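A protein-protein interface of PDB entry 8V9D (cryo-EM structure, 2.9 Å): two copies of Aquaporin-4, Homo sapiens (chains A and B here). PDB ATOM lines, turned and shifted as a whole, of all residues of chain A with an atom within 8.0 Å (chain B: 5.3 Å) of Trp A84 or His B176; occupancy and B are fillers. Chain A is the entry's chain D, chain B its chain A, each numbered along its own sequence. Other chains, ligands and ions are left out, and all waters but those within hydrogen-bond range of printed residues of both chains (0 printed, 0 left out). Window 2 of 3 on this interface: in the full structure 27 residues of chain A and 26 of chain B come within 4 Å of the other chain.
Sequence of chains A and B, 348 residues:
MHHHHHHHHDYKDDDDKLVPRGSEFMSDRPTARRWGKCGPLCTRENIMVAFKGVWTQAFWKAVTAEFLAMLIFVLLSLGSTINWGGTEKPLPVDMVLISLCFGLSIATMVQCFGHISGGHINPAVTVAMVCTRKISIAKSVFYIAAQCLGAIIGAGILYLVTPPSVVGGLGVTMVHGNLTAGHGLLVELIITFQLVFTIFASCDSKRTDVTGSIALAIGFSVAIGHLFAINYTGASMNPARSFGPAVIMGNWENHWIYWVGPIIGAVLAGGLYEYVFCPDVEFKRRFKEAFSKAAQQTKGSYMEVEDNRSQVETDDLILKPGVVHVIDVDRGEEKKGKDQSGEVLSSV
The side-chain amide nitrogen of Asn B231 lies close to the indole nitrogen of Trp A84, 3.5 Å away.
The side-chain hydroxyl (OG1) of Thr A162 lies within hydrogen-bond range of the side-chain hydroxyl (OH) of Tyr B232.
A ring nitrogen (ND1) of His B176 is in hydrogen-bond range of the backbone NH (N) of Asn B178.
The backbone carbonyl oxygen (O) of Tyr B232 is in hydrogen-bond range of the backbone NH (N) of His B176, at 3.0 Å.
Among the printed residues, pairs that only touch across the chains: Ile A82 with Tyr B232 (3.9 Å), Trp A84 with His B176 (3.6 Å), Trp A84 with Tyr B232 (3.7 Å), Val A161 with Leu B179 (3.9 Å), Val A161 with Tyr B232 (3.95 Å) and Pro A163 with Leu B179 (3.5 Å).
Of chain A, only Trp A84 (3.6 Å) comes within 4 Å of His B176.
Of the printed residues of chain A, Leu B179 touches Val A161 and Pro A163.
Of the printed residues of chain B, Pro A163 touches Leu B179.
Printed residues of chain A within 4 Å of Tyr B232: Ile A82, Trp A84, Val A161 and Thr A162.
Thr A81 touches none of the printed residues of chain B.
The nearest residue of chain A that does not touch His B176 is Pro A163 (4.5 Å).
The nearest printed residue of chain B that does not touch Pro A163 is Asn B178 (4.1 Å).
Of the 9 printed residues of chain B, 4 touch a printed residue of chain A.
Printed residues of chain B that touch a printed residue of chain A: His B176, Leu B179, Asn B231 and Tyr B232.
Hydrophobic or aromatic side chains of chain B that line the printed part of chain A: His B176, Leu B179 and Tyr B232.
Of the 20 printed residues of chain A, 5 touch a printed residue of chain B.
Hydrophobic or aromatic side chains of chain A within 4 Å of the printed part of chain B: Ile A82, Trp A84 and Pro A163.
No position is printed for both chains.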
ATOM      1  N   GLY A  79     -29.665  27.838   1.005  1.00  0.00           N
ATOM      2  CA  GLY A  79     -28.237  28.066   0.890  1.00  0.00           C
ATOM      3  C   GLY A  79     -27.843  29.507   1.128  1.00  0.00           C
ATOM      4  O   GLY A  79     -26.769  29.779   1.670  1.00  0.00           O
ATOM      5  N   SER A  80     -28.694  30.450   0.719  1.00  0.00           N
ATOM      6  CA  SER A  80     -28.416  31.863   0.941  1.00  0.00           C
ATOM      7  C   SER A  80     -28.500  32.251   2.411  1.00  0.00           C
ATOM      8  O   SER A  80     -28.001  33.317   2.784  1.00  0.00           O
ATOM      9  CB  SER A  80     -29.380  32.719   0.125  1.00  0.00           C
ATOM     10  OG  SER A  80     -30.600  32.906   0.816  1.00  0.00           O
ATOM     11  N   THR A  81     -29.118  31.421   3.247  1.00  0.00           N
ATOM     12  CA  THR A  81     -29.225  31.697   4.673  1.00  0.00           C
ATOM     13  C   THR A  81     -28.024  31.202   5.465  1.00  0.00           C
ATOM     14  O   THR A  81     -27.948  31.456   6.670  1.00  0.00           O
ATOM     15  CB  THR A  81     -30.499  31.067   5.243  1.00  0.00           C
ATOM     16  OG1 THR A  81     -30.446  29.647   5.078  1.00  0.00           O
ATOM     17  CG2 THR A  81     -31.724  31.608   4.534  1.00  0.00           C
ATOM     18  N   ILE A  82     -27.089  30.502   4.823  1.00  0.00           N
ATOM     19  CA  ILE A  82     -25.921  29.987   5.523  1.00  0.00           C
ATOM     20  C   ILE A  82     -25.051  31.150   5.976  1.00  0.00           C
ATOM     21  O   ILE A  82     -24.783  32.082   5.207  1.00  0.00           O
ATOM     22  CB  ILE A  82     -25.136  29.022   4.623  1.00  0.00           C
ATOM     23  CG1 ILE A  82     -25.949  27.755   4.352  1.00  0.00           C
ATOM     24  CG2 ILE A  82     -23.802  28.671   5.251  1.00  0.00           C
ATOM     25  CD1 ILE A  82     -26.328  26.991   5.590  1.00  0.00           C
ATOM     26  N   ASN A  83     -24.608  31.104   7.229  1.00  0.00           N
ATOM     27  CA  ASN A  83     -23.727  32.126   7.783  1.00  0.00           C
ATOM     28  C   ASN A  83     -22.287  31.671   7.588  1.00  0.00           C
ATOM     29  O   ASN A  83     -21.842  30.703   8.213  1.00  0.00           O
ATOM     30  CB  ASN A  83     -24.040  32.369   9.256  1.00  0.00           C
ATOM     31  CG  ASN A  83     -23.492  33.688   9.758  1.00  0.00           C
ATOM     32  OD1 ASN A  83     -22.326  34.009   9.546  1.00  0.00           O
ATOM     33  ND2 ASN A  83     -24.335  34.461  10.426  1.00  0.00           N
ATOM     34  N   TRP A  84     -21.559  32.369   6.724  1.00  0.00           N
ATOM     35  CA  TRP A  84     -20.215  31.976   6.328  1.00  0.00           C
ATOM     36  C   TRP A  84     -19.141  32.481   7.278  1.00  0.00           C
ATOM     37  O   TRP A  84     -17.961  32.181   7.072  1.00  0.00           O
ATOM     38  CB  TRP A  84     -19.939  32.463   4.905  1.00  0.00           C
ATOM     39  CG  TRP A  84     -20.424  31.499   3.873  1.00  0.00           C
ATOM     40  CD1 TRP A  84     -21.501  31.652   3.057  1.00  0.00           C
ATOM     41  CD2 TRP A  84     -19.832  30.244   3.527  1.00  0.00           C
ATOM     42  NE1 TRP A  84     -21.631  30.560   2.238  1.00  0.00           N
ATOM     43  CE2 TRP A  84     -20.616  29.681   2.504  1.00  0.00           C
ATOM     44  CE3 TRP A  84     -18.720  29.537   3.988  1.00  0.00           C
ATOM     45  CZ2 TRP A  84     -20.323  28.449   1.934  1.00  0.00           C
ATOM     46  CZ3 TRP A  84     -18.431  28.314   3.420  1.00  0.00           C
ATOM     47  CH2 TRP A  84     -19.230  27.782   2.403  1.00  0.00           C
ATOM     48  N   GLY A  85     -19.513  33.239   8.306  1.00  0.00           N
ATOM     49  CA  GLY A  85     -18.562  33.624   9.328  1.00  0.00           C
ATOM     50  C   GLY A  85     -18.310  32.576  10.385  1.00  0.00           C
ATOM     51  O   GLY A  85     -17.452  32.780  11.249  1.00  0.00           O
ATOM     52  N   GLY A  86     -19.036  31.463  10.339  1.00  0.00           N
ATOM     53  CA  GLY A  86     -18.847  30.392  11.293  1.00  0.00           C
ATOM     54  C   GLY A  86     -19.493  30.685  12.631  1.00  0.00           C
ATOM     55  O   GLY A  86     -20.119  31.722  12.854  1.00  0.00           O
ATOM     56  N   THR A  87     -19.336  29.728  13.546  1.00  0.00           N
ATOM     57  CA  THR A  87     -19.849  29.887  14.901  1.00  0.00           C
ATOM     58  C   THR A  87     -18.927  30.718  15.782  1.00  0.00           C
ATOM     59  O   THR A  87     -19.355  31.175  16.846  1.00  0.00           O
ATOM     60  CB  THR A  87     -20.068  28.517  15.547  1.00  0.00           C
ATOM     61  OG1 THR A  87     -20.728  28.682  16.806  1.00  0.00           O
ATOM     62  CG2 THR A  87     -18.740  27.817  15.766  1.00  0.00           C
ATOM     63  N   GLU A  88     -17.681  30.930  15.360  1.00  0.00           N
ATOM     64  CA  GLU A  88     -16.740  31.703  16.163  1.00  0.00           C
ATOM     65  C   GLU A  88     -17.065  33.191  16.105  1.00  0.00           C
ATOM     66  O   GLU A  88     -17.304  33.829  17.137  1.00  0.00           O
ATOM     67  CB  GLU A  88     -15.311  31.431  15.688  1.00  0.00           C
ATOM     68  CG  GLU A  88     -15.038  31.855  14.250  1.00  0.00           C
ATOM     69  CD  GLU A  88     -13.655  31.464  13.774  1.00  0.00           C
ATOM     70  OE1 GLU A  88     -12.790  31.172  14.627  1.00  0.00           O
ATOM     71  OE2 GLU A  88     -13.431  31.455  12.547  1.00  0.00           O
ATOM     72  N   LYS A  89     -17.073  33.764  14.903  1.00  0.00           N
ATOM     73  CA  LYS A  89     -17.365  35.181  14.692  1.00  0.00           C
ATOM     74  C   LYS A  89     -18.396  35.301  13.579  1.00  0.00           C
ATOM     75  O   LYS A  89     -18.045  35.524  12.412  1.00  0.00           O
ATOM     76  CB  LYS A  89     -16.095  35.965  14.359  1.00  0.00           C
ATOM     77  CG  LYS A  89     -16.337  37.444  14.132  1.00  0.00           C
ATOM     78  CD  LYS A  89     -16.762  38.130  15.420  1.00  0.00           C
ATOM     79  CE  LYS A  89     -16.856  39.635  15.241  1.00  0.00           C
ATOM     80  NZ  LYS A  89     -17.953  40.007  14.303  1.00  0.00           N
ATOM     81  N   PRO A  90     -19.677  35.153  13.901  1.00  0.00           N
ATOM     82  CA  PRO A  90     -20.709  35.229  12.861  1.00  0.00           C
ATOM     83  C   PRO A  90     -20.692  36.574  12.151  1.00  0.00           C
ATOM     84  O   PRO A  90     -20.457  37.618  12.760  1.00  0.00           O
ATOM     85  CB  PRO A  90     -22.013  35.021  13.639  1.00  0.00           C
ATOM     86  CG  PRO A  90     -21.611  34.342  14.898  1.00  0.00           C
ATOM     87  CD  PRO A  90     -20.241  34.847  15.225  1.00  0.00           C
ATOM     88  N   LEU A  91     -20.946  36.536  10.846  1.00  0.00           N
ATOM     89  CA  LEU A  91     -21.066  37.748  10.054  1.00  0.00           C
ATOM     90  C   LEU A  91     -22.449  38.368  10.236  1.00  0.00           C
ATOM     91  O   LEU A  91     -23.409  37.672  10.578  1.00  0.00           O
ATOM     92  CB  LEU A  91     -20.835  37.445   8.577  1.00  0.00           C
ATOM     93  CG  LEU A  91     -19.397  37.209   8.123  1.00  0.00           C
ATOM     94  CD1 LEU A  91     -19.368  36.758   6.675  1.00  0.00           C
ATOM     95  CD2 LEU A  91     -18.568  38.464   8.310  1.00  0.00           C
ATOM     96  N   PRO A  92     -22.577  39.675  10.022  1.00  0.00           N
ATOM     97  CA  PRO A  92     -23.906  40.295  10.074  1.00  0.00           C
ATOM     98  C   PRO A  92     -24.833  39.676   9.038  1.00  0.00           C
ATOM     99  O   PRO A  92     -24.417  39.340   7.926  1.00  0.00           O
ATOM    100  CB  PRO A  92     -23.628  41.772   9.773  1.00  0.00           C
ATOM    101  CG  PRO A  92     -22.221  41.835   9.285  1.00  0.00           C
ATOM    102  CD  PRO A  92     -21.505  40.666   9.855  1.00  0.00           C
ATOM    103  N   VAL A 161     -23.196  19.220   0.832  1.00  0.00           N
ATOM    104  CA  VAL A 161     -22.198  20.074   0.190  1.00  0.00           C
ATOM    105  C   VAL A 161     -21.692  21.187   1.095  1.00  0.00           C
ATOM    106  O   VAL A 161     -20.680  21.824   0.767  1.00  0.00           O
ATOM    107  CB  VAL A 161     -22.746  20.700  -1.108  1.00  0.00           C
ATOM    108  CG1 VAL A 161     -23.192  19.618  -2.075  1.00  0.00           C
ATOM    109  CG2 VAL A 161     -23.888  21.653  -0.801  1.00  0.00           C
ATOM    110  N   THR A 162     -22.353  21.444   2.213  1.00  0.00           N
ATOM    111  CA  THR A 162     -21.957  22.533   3.100  1.00  0.00           C
ATOM    112  C   THR A 162     -20.904  22.052   4.091  1.00  0.00           C
ATOM    113  O   THR A 162     -21.089  21.003   4.717  1.00  0.00           O
ATOM    114  CB  THR A 162     -23.157  23.077   3.860  1.00  0.00           C
ATOM    115  OG1 THR A 162     -24.249  23.267   2.955  1.00  0.00           O
ATOM    116  CG2 THR A 162     -22.815  24.405   4.505  1.00  0.00           C
ATOM    117  N   PRO A 163     -19.801  22.775   4.258  1.00  0.00           N
ATOM    118  CA  PRO A 163     -18.804  22.389   5.259  1.00  0.00           C
ATOM    119  C   PRO A 163     -19.415  22.361   6.647  1.00  0.00           C
ATOM    120  O   PRO A 163     -20.270  23.195   6.976  1.00  0.00           O
ATOM    121  CB  PRO A 163     -17.740  23.490   5.140  1.00  0.00           C
ATOM    122  CG  PRO A 163     -17.910  24.033   3.771  1.00  0.00           C
ATOM    123  CD  PRO A 163     -19.373  23.946   3.475  1.00  0.00           C
ATOM    124  N   SER A 165     -18.471  23.400   9.383  1.00  0.00           N
ATOM    125  CA  SER A 165     -18.212  24.560  10.226  1.00  0.00           C
ATOM    126  C   SER A 165     -19.276  25.641  10.083  1.00  0.00           C
ATOM    127  O   SER A 165     -19.424  26.465  10.989  1.00  0.00           O
ATOM    128  CB  SER A 165     -16.838  25.146   9.901  1.00  0.00           C
ATOM    129  OG  SER A 165     -15.864  24.125   9.781  1.00  0.00           O
ATOM    130  N   VAL A 166     -20.017  25.658   8.975  1.00  0.00           N
ATOM    131  CA  VAL A 166     -20.967  26.725   8.688  1.00  0.00           C
ATOM    132  C   VAL A 166     -22.394  26.220   8.541  1.00  0.00           C
ATOM    133  O   VAL A 166     -23.282  27.010   8.211  1.00  0.00           O
ATOM    134  CB  VAL A 166     -20.557  27.515   7.430  1.00  0.00           C
ATOM    135  CG1 VAL A 166     -19.163  28.091   7.593  1.00  0.00           C
ATOM    136  CG2 VAL A 166     -20.631  26.628   6.202  1.00  0.00           C
ATOM    137  N   VAL A 167     -22.645  24.933   8.780  1.00  0.00           N
ATOM    138  CA  VAL A 167     -23.989  24.396   8.586  1.00  0.00           C
ATOM    139  C   VAL A 167     -24.982  25.118   9.488  1.00  0.00           C
ATOM    140  O   VAL A 167     -26.059  25.535   9.049  1.00  0.00           O
ATOM    141  CB  VAL A 167     -24.001  22.877   8.832  1.00  0.00           C
ATOM    142  CG1 VAL A 167     -25.421  22.380   9.004  1.00  0.00           C
ATOM    143  CG2 VAL A 167     -23.315  22.152   7.693  1.00  0.00           C
ATOM    144  N   MET B 174     -13.020  30.248  -7.901  1.00  0.00           N
ATOM    145  CA  MET B 174     -12.284  29.211  -7.194  1.00  0.00           C
ATOM    146  C   MET B 174     -13.236  28.415  -6.316  1.00  0.00           C
ATOM    147  O   MET B 174     -14.241  28.937  -5.830  1.00  0.00           O
ATOM    148  CB  MET B 174     -11.164  29.782  -6.317  1.00  0.00           C
ATOM    149  CG  MET B 174     -10.032  30.438  -7.068  1.00  0.00           C
ATOM    150  SD  MET B 174      -8.759  31.002  -5.928  1.00  0.00           S
ATOM    151  CE  MET B 174      -9.562  32.430  -5.209  1.00  0.00           C
ATOM    152  N   VAL B 175     -12.904  27.146  -6.116  1.00  0.00           N
ATOM    153  CA  VAL B 175     -13.660  26.295  -5.207  1.00  0.00           C
ATOM    154  C   VAL B 175     -13.246  26.603  -3.776  1.00  0.00           C
ATOM    155  O   VAL B 175     -12.078  26.892  -3.490  1.00  0.00           O
ATOM    156  CB  VAL B 175     -13.449  24.807  -5.545  1.00  0.00           C
ATOM    157  CG1 VAL B 175     -14.227  23.937  -4.587  1.00  0.00           C
ATOM    158  CG2 VAL B 175     -13.866  24.524  -6.971  1.00  0.00           C
ATOM    159  N   HIS B 176     -14.211  26.546  -2.864  1.00  0.00           N
ATOM    160  CA  HIS B 176     -13.924  26.835  -1.468  1.00  0.00           C
ATOM    161  C   HIS B 176     -12.895  25.845  -0.936  1.00  0.00           C
ATOM    162  O   HIS B 176     -12.840  24.688  -1.354  1.00  0.00           O
ATOM    163  CB  HIS B 176     -15.206  26.774  -0.640  1.00  0.00           C
ATOM    164  CG  HIS B 176     -15.045  27.248   0.770  1.00  0.00           C
ATOM    165  ND1 HIS B 176     -14.637  26.421   1.794  1.00  0.00           N
ATOM    166  CD2 HIS B 176     -15.250  28.463   1.330  1.00  0.00           C
ATOM    167  CE1 HIS B 176     -14.592  27.107   2.921  1.00  0.00           C
ATOM    168  NE2 HIS B 176     -14.960  28.350   2.667  1.00  0.00           N
ATOM    169  N   GLY B 177     -12.064  26.317  -0.006  1.00  0.00           N
ATOM    170  CA  GLY B 177     -10.977  25.486   0.481  1.00  0.00           C
ATOM    171  C   GLY B 177     -11.458  24.189   1.100  1.00  0.00           C
ATOM    172  O   GLY B 177     -10.822  23.143   0.944  1.00  0.00           O
ATOM    173  N   ASN B 178     -12.586  24.235   1.805  1.00  0.00           N
ATOM    174  CA  ASN B 178     -13.095  23.077   2.529  1.00  0.00           C
ATOM    175  C   ASN B 178     -14.001  22.182   1.691  1.00  0.00           C
ATOM    176  O   ASN B 178     -14.493  21.178   2.213  1.00  0.00           O
ATOM    177  CB  ASN B 178     -13.847  23.534   3.780  1.00  0.00           C
ATOM    178  CG  ASN B 178     -12.923  24.097   4.840  1.00  0.00           C
ATOM    179  OD1 ASN B 178     -11.855  23.548   5.103  1.00  0.00           O
ATOM    180  ND2 ASN B 178     -13.335  25.191   5.462  1.00  0.00           N
ATOM    181  N   LEU B 179     -14.237  22.509   0.425  1.00  0.00           N
ATOM    182  CA  LEU B 179     -15.085  21.708  -0.448  1.00  0.00           C
ATOM    183  C   LEU B 179     -14.228  20.887  -1.398  1.00  0.00           C
ATOM    184  O   LEU B 179     -13.300  21.415  -2.018  1.00  0.00           O
ATOM    185  CB  LEU B 179     -16.049  22.582  -1.255  1.00  0.00           C
ATOM    186  CG  LEU B 179     -17.294  23.137  -0.566  1.00  0.00           C
ATOM    187  CD1 LEU B 179     -16.942  24.225   0.425  1.00  0.00           C
ATOM    188  CD2 LEU B 179     -18.262  23.651  -1.614  1.00  0.00           C
ATOM    189  N   ASN B 231     -19.911  31.672  -2.454  1.00  0.00           N
ATOM    190  CA  ASN B 231     -18.950  31.165  -1.485  1.00  0.00           C
ATOM    191  C   ASN B 231     -18.700  29.668  -1.607  1.00  0.00           C
ATOM    192  O   ASN B 231     -17.852  29.140  -0.885  1.00  0.00           O
ATOM    193  CB  ASN B 231     -19.408  31.494  -0.061  1.00  0.00           C
ATOM    194  CG  ASN B 231     -19.301  32.971   0.262  1.00  0.00           C
ATOM    195  OD1 ASN B 231     -18.318  33.622  -0.083  1.00  0.00           O
ATOM    196  ND2 ASN B 231     -20.311  33.504   0.931  1.00  0.00           N
ATOM    197  N   TYR B 232     -19.405  28.973  -2.498  1.00  0.00           N
ATOM    198  CA  TYR B 232     -19.152  27.552  -2.717  1.00  0.00           C
ATOM    199  C   TYR B 232     -18.137  27.332  -3.834  1.00  0.00           C
ATOM    200  O   TYR B 232     -17.091  26.714  -3.618  1.00  0.00           O
ATOM    201  CB  TYR B 232     -20.458  26.816  -3.039  1.00  0.00           C
ATOM    202  CG  TYR B 232     -21.399  26.660  -1.868  1.00  0.00           C
ATOM    203  CD1 TYR B 232     -22.222  27.699  -1.470  1.00  0.00           C
ATOM    204  CD2 TYR B 232     -21.456  25.472  -1.159  1.00  0.00           C
ATOM    205  CE1 TYR B 232     -23.080  27.557  -0.402  1.00  0.00           C
ATOM    206  CE2 TYR B 232     -22.307  25.322  -0.089  1.00  0.00           C
ATOM    207  CZ  TYR B 232     -23.117  26.365   0.285  1.00  0.00           C
ATOM    208  OH  TYR B 232     -23.968  26.214   1.351  1.00  0.00           O
ATOM    209  N   THR B 233     -18.437  27.831  -5.036  1.00  0.00           N
ATOM    210  CA  THR B 233     -17.571  27.634  -6.191  1.00  0.00           C
ATOM    211  C   THR B 233     -17.378  28.899  -7.017  1.00  0.00           C
ATOM    212  O   THR B 233     -16.784  28.830  -8.098  1.00  0.00           O
ATOM    213  CB  THR B 233     -18.120  26.520  -7.089  1.00  0.00           C
ATOM    214  OG1 THR B 233     -19.396  26.912  -7.609  1.00  0.00           O
ATOM    215  CG2 THR B 233     -18.271  25.228  -6.312  1.00  0.00           C
